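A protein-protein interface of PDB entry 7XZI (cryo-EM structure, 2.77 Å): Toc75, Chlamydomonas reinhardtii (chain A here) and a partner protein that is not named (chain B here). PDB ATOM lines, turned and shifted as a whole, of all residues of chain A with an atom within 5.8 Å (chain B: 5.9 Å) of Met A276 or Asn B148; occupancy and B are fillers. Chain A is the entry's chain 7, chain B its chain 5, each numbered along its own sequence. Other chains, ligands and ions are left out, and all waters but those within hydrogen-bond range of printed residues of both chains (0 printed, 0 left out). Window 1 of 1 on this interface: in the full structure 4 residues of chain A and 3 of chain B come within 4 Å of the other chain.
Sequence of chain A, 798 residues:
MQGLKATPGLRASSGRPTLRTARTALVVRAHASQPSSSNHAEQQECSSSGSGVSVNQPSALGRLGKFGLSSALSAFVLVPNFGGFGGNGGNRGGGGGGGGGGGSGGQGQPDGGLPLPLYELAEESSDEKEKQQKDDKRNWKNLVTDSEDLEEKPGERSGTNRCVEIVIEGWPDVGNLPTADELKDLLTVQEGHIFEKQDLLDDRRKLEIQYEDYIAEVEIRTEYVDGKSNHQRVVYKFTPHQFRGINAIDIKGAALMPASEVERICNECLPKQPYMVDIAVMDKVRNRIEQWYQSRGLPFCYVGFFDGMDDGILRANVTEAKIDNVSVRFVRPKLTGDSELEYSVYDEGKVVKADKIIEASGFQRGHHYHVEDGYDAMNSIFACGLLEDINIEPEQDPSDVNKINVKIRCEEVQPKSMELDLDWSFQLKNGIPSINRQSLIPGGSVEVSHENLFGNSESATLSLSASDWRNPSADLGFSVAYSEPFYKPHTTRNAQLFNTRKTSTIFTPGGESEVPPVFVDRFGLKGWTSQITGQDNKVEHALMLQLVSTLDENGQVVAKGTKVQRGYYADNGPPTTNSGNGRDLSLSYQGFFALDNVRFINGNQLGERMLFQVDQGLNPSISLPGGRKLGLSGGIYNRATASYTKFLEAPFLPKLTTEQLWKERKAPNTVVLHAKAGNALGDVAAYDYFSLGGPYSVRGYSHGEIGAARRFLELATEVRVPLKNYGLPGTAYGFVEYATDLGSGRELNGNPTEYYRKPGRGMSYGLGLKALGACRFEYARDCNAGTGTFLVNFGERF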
ATOM      1  N   GLN A 242       1.893 -16.225   2.714  1.00  0.00           N
ATOM      2  CA  GLN A 242       2.653 -14.993   2.845  1.00  0.00           C
ATOM      3  C   GLN A 242       4.128 -15.246   2.564  1.00  0.00           C
ATOM      4  O   GLN A 242       4.615 -16.376   2.647  1.00  0.00           O
ATOM      5  CB  GLN A 242       2.493 -14.380   4.241  1.00  0.00           C
ATOM      6  CG  GLN A 242       1.072 -13.972   4.588  1.00  0.00           C
ATOM      7  CD  GLN A 242       0.922 -13.554   6.036  1.00  0.00           C
ATOM      8  OE1 GLN A 242       1.762 -13.875   6.877  1.00  0.00           O
ATOM      9  NE2 GLN A 242      -0.149 -12.830   6.334  1.00  0.00           N
ATOM     10  N   PHE A 243       4.830 -14.169   2.225  1.00  0.00           N
ATOM     11  CA  PHE A 243       6.278 -14.169   2.070  1.00  0.00           C
ATOM     12  C   PHE A 243       6.897 -13.503   3.290  1.00  0.00           C
ATOM     13  O   PHE A 243       6.332 -12.545   3.829  1.00  0.00           O
ATOM     14  CB  PHE A 243       6.709 -13.430   0.801  1.00  0.00           C
ATOM     15  CG  PHE A 243       6.312 -14.118  -0.472  1.00  0.00           C
ATOM     16  CD1 PHE A 243       6.859 -15.342  -0.815  1.00  0.00           C
ATOM     17  CD2 PHE A 243       5.409 -13.527  -1.339  1.00  0.00           C
ATOM     18  CE1 PHE A 243       6.501 -15.972  -1.989  1.00  0.00           C
ATOM     19  CE2 PHE A 243       5.048 -14.150  -2.516  1.00  0.00           C
ATOM     20  CZ  PHE A 243       5.594 -15.376  -2.841  1.00  0.00           C
ATOM     21  N   ARG A 244       8.053 -14.013   3.724  1.00  0.00           N
ATOM     22  CA  ARG A 244       8.712 -13.449   4.898  1.00  0.00           C
ATOM     23  C   ARG A 244       9.079 -11.984   4.695  1.00  0.00           C
ATOM     24  O   ARG A 244       9.060 -11.203   5.653  1.00  0.00           O
ATOM     25  CB  ARG A 244       9.955 -14.269   5.250  1.00  0.00           C
ATOM     26  CG  ARG A 244       9.646 -15.592   5.927  1.00  0.00           C
ATOM     27  CD  ARG A 244      10.916 -16.340   6.288  1.00  0.00           C
ATOM     28  NE  ARG A 244      10.625 -17.557   7.031  1.00  0.00           N
ATOM     29  CZ  ARG A 244      10.310 -18.719   6.470  1.00  0.00           C
ATOM     30  NH1 ARG A 244      10.247 -18.856   5.155  1.00  0.00           N
ATOM     31  NH2 ARG A 244      10.047 -19.764   7.246  1.00  0.00           N
ATOM     32  N   GLY A 245       9.420 -11.592   3.470  1.00  0.00           N
ATOM     33  CA  GLY A 245       9.687 -10.193   3.196  1.00  0.00           C
ATOM     34  C   GLY A 245       9.724  -9.822   1.727  1.00  0.00           C
ATOM     35  O   GLY A 245      10.410 -10.466   0.929  1.00  0.00           O
ATOM     36  N   GLN A 273       3.228  -2.956   3.637  1.00  0.00           N
ATOM     37  CA  GLN A 273       4.127  -3.366   4.701  1.00  0.00           C
ATOM     38  C   GLN A 273       5.218  -4.271   4.146  1.00  0.00           C
ATOM     39  O   GLN A 273       4.927  -5.156   3.330  1.00  0.00           O
ATOM     40  CB  GLN A 273       3.352  -4.099   5.813  1.00  0.00           C
ATOM     41  CG  GLN A 273       4.205  -4.546   6.990  1.00  0.00           C
ATOM     42  CD  GLN A 273       3.396  -5.256   8.057  1.00  0.00           C
ATOM     43  OE1 GLN A 273       2.178  -5.391   7.941  1.00  0.00           O
ATOM     44  NE2 GLN A 273       4.069  -5.713   9.106  1.00  0.00           N
ATOM     45  N   PRO A 274       6.476  -4.086   4.552  1.00  0.00           N
ATOM     46  CA  PRO A 274       7.567  -4.923   4.039  1.00  0.00           C
ATOM     47  C   PRO A 274       7.711  -6.277   4.716  1.00  0.00           C
ATOM     48  O   PRO A 274       8.634  -7.020   4.370  1.00  0.00           O
ATOM     49  CB  PRO A 274       8.803  -4.053   4.303  1.00  0.00           C
ATOM     50  CG  PRO A 274       8.442  -3.266   5.510  1.00  0.00           C
ATOM     51  CD  PRO A 274       6.972  -2.973   5.380  1.00  0.00           C
ATOM     52  N   TYR A 275       6.843  -6.626   5.664  1.00  0.00           N
ATOM     53  CA  TYR A 275       6.926  -7.896   6.373  1.00  0.00           C
ATOM     54  C   TYR A 275       5.624  -8.668   6.221  1.00  0.00           C
ATOM     55  O   TYR A 275       4.537  -8.081   6.226  1.00  0.00           O
ATOM     56  CB  TYR A 275       7.234  -7.689   7.860  1.00  0.00           C
ATOM     57  CG  TYR A 275       8.636  -7.194   8.141  1.00  0.00           C
ATOM     58  CD1 TYR A 275       9.734  -8.030   7.980  1.00  0.00           C
ATOM     59  CD2 TYR A 275       8.859  -5.898   8.583  1.00  0.00           C
ATOM     60  CE1 TYR A 275      11.016  -7.583   8.239  1.00  0.00           C
ATOM     61  CE2 TYR A 275      10.137  -5.443   8.846  1.00  0.00           C
ATOM     62  CZ  TYR A 275      11.210  -6.289   8.673  1.00  0.00           C
ATOM     63  OH  TYR A 275      12.484  -5.838   8.935  1.00  0.00           O
ATOM     64  N   MET A 276       5.749  -9.992   6.089  1.00  0.00           N
ATOM     65  CA  MET A 276       4.603 -10.899   5.986  1.00  0.00           C
ATOM     66  C   MET A 276       3.688 -10.516   4.824  1.00  0.00           C
ATOM     67  O   MET A 276       2.466 -10.443   4.968  1.00  0.00           O
ATOM     68  CB  MET A 276       3.824 -10.955   7.302  1.00  0.00           C
ATOM     69  CG  MET A 276       4.699 -11.159   8.530  1.00  0.00           C
ATOM     70  SD  MET A 276       5.723 -12.643   8.450  1.00  0.00           S
ATOM     71  CE  MET A 276       4.483 -13.926   8.587  1.00  0.00           C
ATOM     72  N   VAL A 277       4.287 -10.267   3.659  1.00  0.00           N
ATOM     73  CA  VAL A 277       3.515  -9.888   2.482  1.00  0.00           C
ATOM     74  C   VAL A 277       2.874 -11.122   1.865  1.00  0.00           C
ATOM     75  O   VAL A 277       3.530 -12.151   1.656  1.00  0.00           O
ATOM     76  CB  VAL A 277       4.411  -9.163   1.462  1.00  0.00           C
ATOM     77  CG1 VAL A 277       3.567  -8.565   0.347  1.00  0.00           C
ATOM     78  CG2 VAL A 277       5.241  -8.095   2.151  1.00  0.00           C
ATOM     79  N   ASP A 278       1.583 -11.020   1.556  1.00  0.00           N
ATOM     80  CA  ASP A 278       0.863 -12.127   0.949  1.00  0.00           C
ATOM     81  C   ASP A 278       1.315 -12.339  -0.496  1.00  0.00           C
ATOM     82  O   ASP A 278       2.016 -11.513  -1.086  1.00  0.00           O
ATOM     83  CB  ASP A 278      -0.645 -11.881   1.002  1.00  0.00           C
ATOM     84  CG  ASP A 278      -1.047 -10.590   0.321  1.00  0.00           C
ATOM     85  OD1 ASP A 278      -0.219  -9.657   0.276  1.00  0.00           O
ATOM     86  OD2 ASP A 278      -2.194 -10.507  -0.167  1.00  0.00           O
ATOM     87  N   TYR B 143      14.920 -10.892  19.651  1.00  0.00           N
ATOM     88  CA  TYR B 143      13.564 -10.403  19.887  1.00  0.00           C
ATOM     89  C   TYR B 143      13.039  -9.638  18.679  1.00  0.00           C
ATOM     90  O   TYR B 143      11.839  -9.680  18.383  1.00  0.00           O
ATOM     91  CB  TYR B 143      13.516  -9.539  21.148  1.00  0.00           C
ATOM     92  CG  TYR B 143      14.118  -8.161  20.997  1.00  0.00           C
ATOM     93  CD1 TYR B 143      15.483  -7.963  21.130  1.00  0.00           C
ATOM     94  CD2 TYR B 143      13.317  -7.057  20.734  1.00  0.00           C
ATOM     95  CE1 TYR B 143      16.035  -6.706  20.997  1.00  0.00           C
ATOM     96  CE2 TYR B 143      13.862  -5.796  20.599  1.00  0.00           C
ATOM     97  CZ  TYR B 143      15.223  -5.627  20.733  1.00  0.00           C
ATOM     98  OH  TYR B 143      15.774  -4.373  20.600  1.00  0.00           O
ATOM     99  N   GLU B 144      13.921  -8.941  17.959  1.00  0.00           N
ATOM    100  CA  GLU B 144      13.510  -8.300  16.714  1.00  0.00           C
ATOM    101  C   GLU B 144      13.092  -9.333  15.675  1.00  0.00           C
ATOM    102  O   GLU B 144      12.116  -9.129  14.941  1.00  0.00           O
ATOM    103  CB  GLU B 144      14.643  -7.422  16.178  1.00  0.00           C
ATOM    104  CG  GLU B 144      15.039  -6.289  17.113  1.00  0.00           C
ATOM    105  CD  GLU B 144      16.187  -5.458  16.573  1.00  0.00           C
ATOM    106  OE1 GLU B 144      16.857  -5.911  15.623  1.00  0.00           O
ATOM    107  OE2 GLU B 144      16.417  -4.349  17.099  1.00  0.00           O
ATOM    108  N   VAL B 145      13.817 -10.451  15.601  1.00  0.00           N
ATOM    109  CA  VAL B 145      13.439 -11.523  14.686  1.00  0.00           C
ATOM    110  C   VAL B 145      12.076 -12.087  15.062  1.00  0.00           C
ATOM    111  O   VAL B 145      11.230 -12.335  14.195  1.00  0.00           O
ATOM    112  CB  VAL B 145      14.523 -12.617  14.669  1.00  0.00           C
ATOM    113  CG1 VAL B 145      14.076 -13.792  13.822  1.00  0.00           C
ATOM    114  CG2 VAL B 145      15.831 -12.050  14.146  1.00  0.00           C
ATOM    115  N   LEU B 146      11.838 -12.295  16.358  1.00  0.00           N
ATOM    116  CA  LEU B 146      10.534 -12.779  16.801  1.00  0.00           C
ATOM    117  C   LEU B 146       9.427 -11.780  16.488  1.00  0.00           C
ATOM    118  O   LEU B 146       8.307 -12.183  16.154  1.00  0.00           O
ATOM    119  CB  LEU B 146      10.561 -13.084  18.299  1.00  0.00           C
ATOM    120  CG  LEU B 146      11.398 -14.279  18.759  1.00  0.00           C
ATOM    121  CD1 LEU B 146      11.306 -14.444  20.269  1.00  0.00           C
ATOM    122  CD2 LEU B 146      10.954 -15.548  18.051  1.00  0.00           C
ATOM    123  N   GLN B 147       9.715 -10.482  16.599  1.00  0.00           N
ATOM    124  CA  GLN B 147       8.717  -9.469  16.277  1.00  0.00           C
ATOM    125  C   GLN B 147       8.410  -9.418  14.785  1.00  0.00           C
ATOM    126  O   GLN B 147       7.259  -9.182  14.402  1.00  0.00           O
ATOM    127  CB  GLN B 147       9.187  -8.092  16.751  1.00  0.00           C
ATOM    128  CG  GLN B 147       9.195  -7.902  18.256  1.00  0.00           C
ATOM    129  CD  GLN B 147       9.649  -6.512  18.657  1.00  0.00           C
ATOM    130  OE1 GLN B 147      10.032  -5.705  17.810  1.00  0.00           O
ATOM    131  NE2 GLN B 147       9.608  -6.226  19.951  1.00  0.00           N
ATOM    132  N   ASN B 148       9.413  -9.627  13.933  1.00  0.00           N
ATOM    133  CA  ASN B 148       9.230  -9.351  12.512  1.00  0.00           C
ATOM    134  C   ASN B 148       9.011 -10.606  11.674  1.00  0.00           C
ATOM    135  O   ASN B 148       7.996 -10.723  10.981  1.00  0.00           O
ATOM    136  CB  ASN B 148      10.435  -8.578  11.971  1.00  0.00           C
ATOM    137  CG  ASN B 148      10.642  -7.252  12.676  1.00  0.00           C
ATOM    138  OD1 ASN B 148       9.697  -6.653  13.189  1.00  0.00           O
ATOM    139  ND2 ASN B 148      11.884  -6.783  12.701  1.00  0.00           N
ATOM    140  N   TYR B 149       9.950 -11.553  11.730  1.00  0.00           N
ATOM    141  CA  TYR B 149       9.924 -12.669  10.789  1.00  0.00           C
ATOM    142  C   TYR B 149       9.131 -13.855  11.329  1.00  0.00           C
ATOM    143  O   TYR B 149       8.473 -14.566  10.559  1.00  0.00           O
ATOM    144  CB  TYR B 149      11.352 -13.094  10.447  1.00  0.00           C
ATOM    145  CG  TYR B 149      12.056 -12.156   9.495  1.00  0.00           C
ATOM    146  CD1 TYR B 149      11.916 -12.301   8.123  1.00  0.00           C
ATOM    147  CD2 TYR B 149      12.863 -11.129   9.967  1.00  0.00           C
ATOM    148  CE1 TYR B 149      12.557 -11.451   7.245  1.00  0.00           C
ATOM    149  CE2 TYR B 149      13.510 -10.271   9.095  1.00  0.00           C
ATOM    150  CZ  TYR B 149      13.353 -10.437   7.735  1.00  0.00           C
ATOM    151  OH  TYR B 149      13.993  -9.588   6.862  1.00  0.00           O
ATOM    152  N   THR B 150       9.181 -14.090  12.635  1.00  0.00           N
ATOM    153  CA  THR B 150       8.600 -15.304  13.192  1.00  0.00           C
ATOM    154  C   THR B 150       7.080 -15.287  13.047  1.00  0.00           C
ATOM    155  O   THR B 150       6.433 -14.314  13.458  1.00  0.00           O
ATOM    156  CB  THR B 150       8.981 -15.455  14.665  1.00  0.00           C
ATOM    157  OG1 THR B 150      10.404 -15.565  14.782  1.00  0.00           O
ATOM    158  CG2 THR B 150       8.333 -16.695  15.260  1.00  0.00           C
ATOM    159  N   PRO B 151       6.479 -16.326  12.474  1.00  0.00           N
ATOM    160  CA  PRO B 151       5.016 -16.385  12.399  1.00  0.00           C
ATOM    161  C   PRO B 151       4.402 -16.614  13.771  1.00  0.00           C
ATOM    162  O   PRO B 151       5.040 -17.116  14.698  1.00  0.00           O
ATOM    163  CB  PRO B 151       4.755 -17.572  11.466  1.00  0.00           C
ATOM    164  CG  PRO B 151       5.960 -18.436  11.623  1.00  0.00           C
ATOM    165  CD  PRO B 151       7.113 -17.493  11.836  1.00  0.00           C
ATOM    166  N   ARG B 186       5.374  -6.933  17.772  1.00  0.00           N
ATOM    167  CA  ARG B 186       5.693  -5.665  17.123  1.00  0.00           C
ATOM    168  C   ARG B 186       4.901  -4.497  17.696  1.00  0.00           C
ATOM    169  O   ARG B 186       5.414  -3.374  17.735  1.00  0.00           O
ATOM    170  CB  ARG B 186       5.444  -5.775  15.617  1.00  0.00           C
ATOM    171  CG  ARG B 186       6.051  -4.646  14.802  1.00  0.00           C
ATOM    172  CD  ARG B 186       5.690  -4.752  13.324  1.00  0.00           C
ATOM    173  NE  ARG B 186       6.139  -6.002  12.726  1.00  0.00           N
ATOM    174  CZ  ARG B 186       5.342  -7.026  12.437  1.00  0.00           C
ATOM    175  NH1 ARG B 186       4.042  -6.979  12.676  1.00  0.00           N
ATOM    176  NH2 ARG B 186       5.863  -8.120  11.891  1.00  0.00           N
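Among the printed residues, merely in contact across the chains: Arg A244 with Tyr B149 (3.9 Å), Gln A273 with Arg B186 (3.8 Å), Tyr A275 with Asn B148 (3.9 Å), Tyr A275 with Tyr B149 (3.7 Å), Met A276 with Asn B148 (3.9 Å) and Met A276 with Tyr B149 (3.96 Å).
Hydrophobic or aromatic side chains of chain B that line the printed part of chain A: Tyr B149. Printed residues of chain A that touch a printed residue of chain B: Arg A244, Gln A273, Tyr A275 and Met A276. Hydrophobic or aromatic side chains of chain A that line the printed part of chain B: Tyr A275 and Met A276.
The backbone carbonyl oxygen (O) of Glu B144 is in hydrogen-bond range of the side-chain amide nitrogen (ND2) of Asn B148, 3.3 Å away. The backbone carbonyl oxygen (O) of Gln B147 sits at hydrogen-bond distance from the guanidinium group (NH2) of Arg B186 (3.1 Å). O of Asn B148 lies within hydrogen-bond range of NH2 of Arg B186, 3.5 Å away. The backbone NH (N) of Met A276 sits close to the backbone carbonyl oxygen (O) of Phe A243.
Printed residues of chain B within 4 Å of Arg A244: Tyr B149. Of chain B, only Asn B148 and Tyr B149 come within 4 Å of Met A276. Val B145 touches none of the printed residues of chain A. Asn B148 touches just these residues of chain A: Tyr A275 (3.9 Å) and Met A276 (3.9 Å). Printed residues of chain A within 4 Å of Tyr B149: Arg A244, Tyr A275 and Met A276. Thr B150 touches none of the printed residues of chain A.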
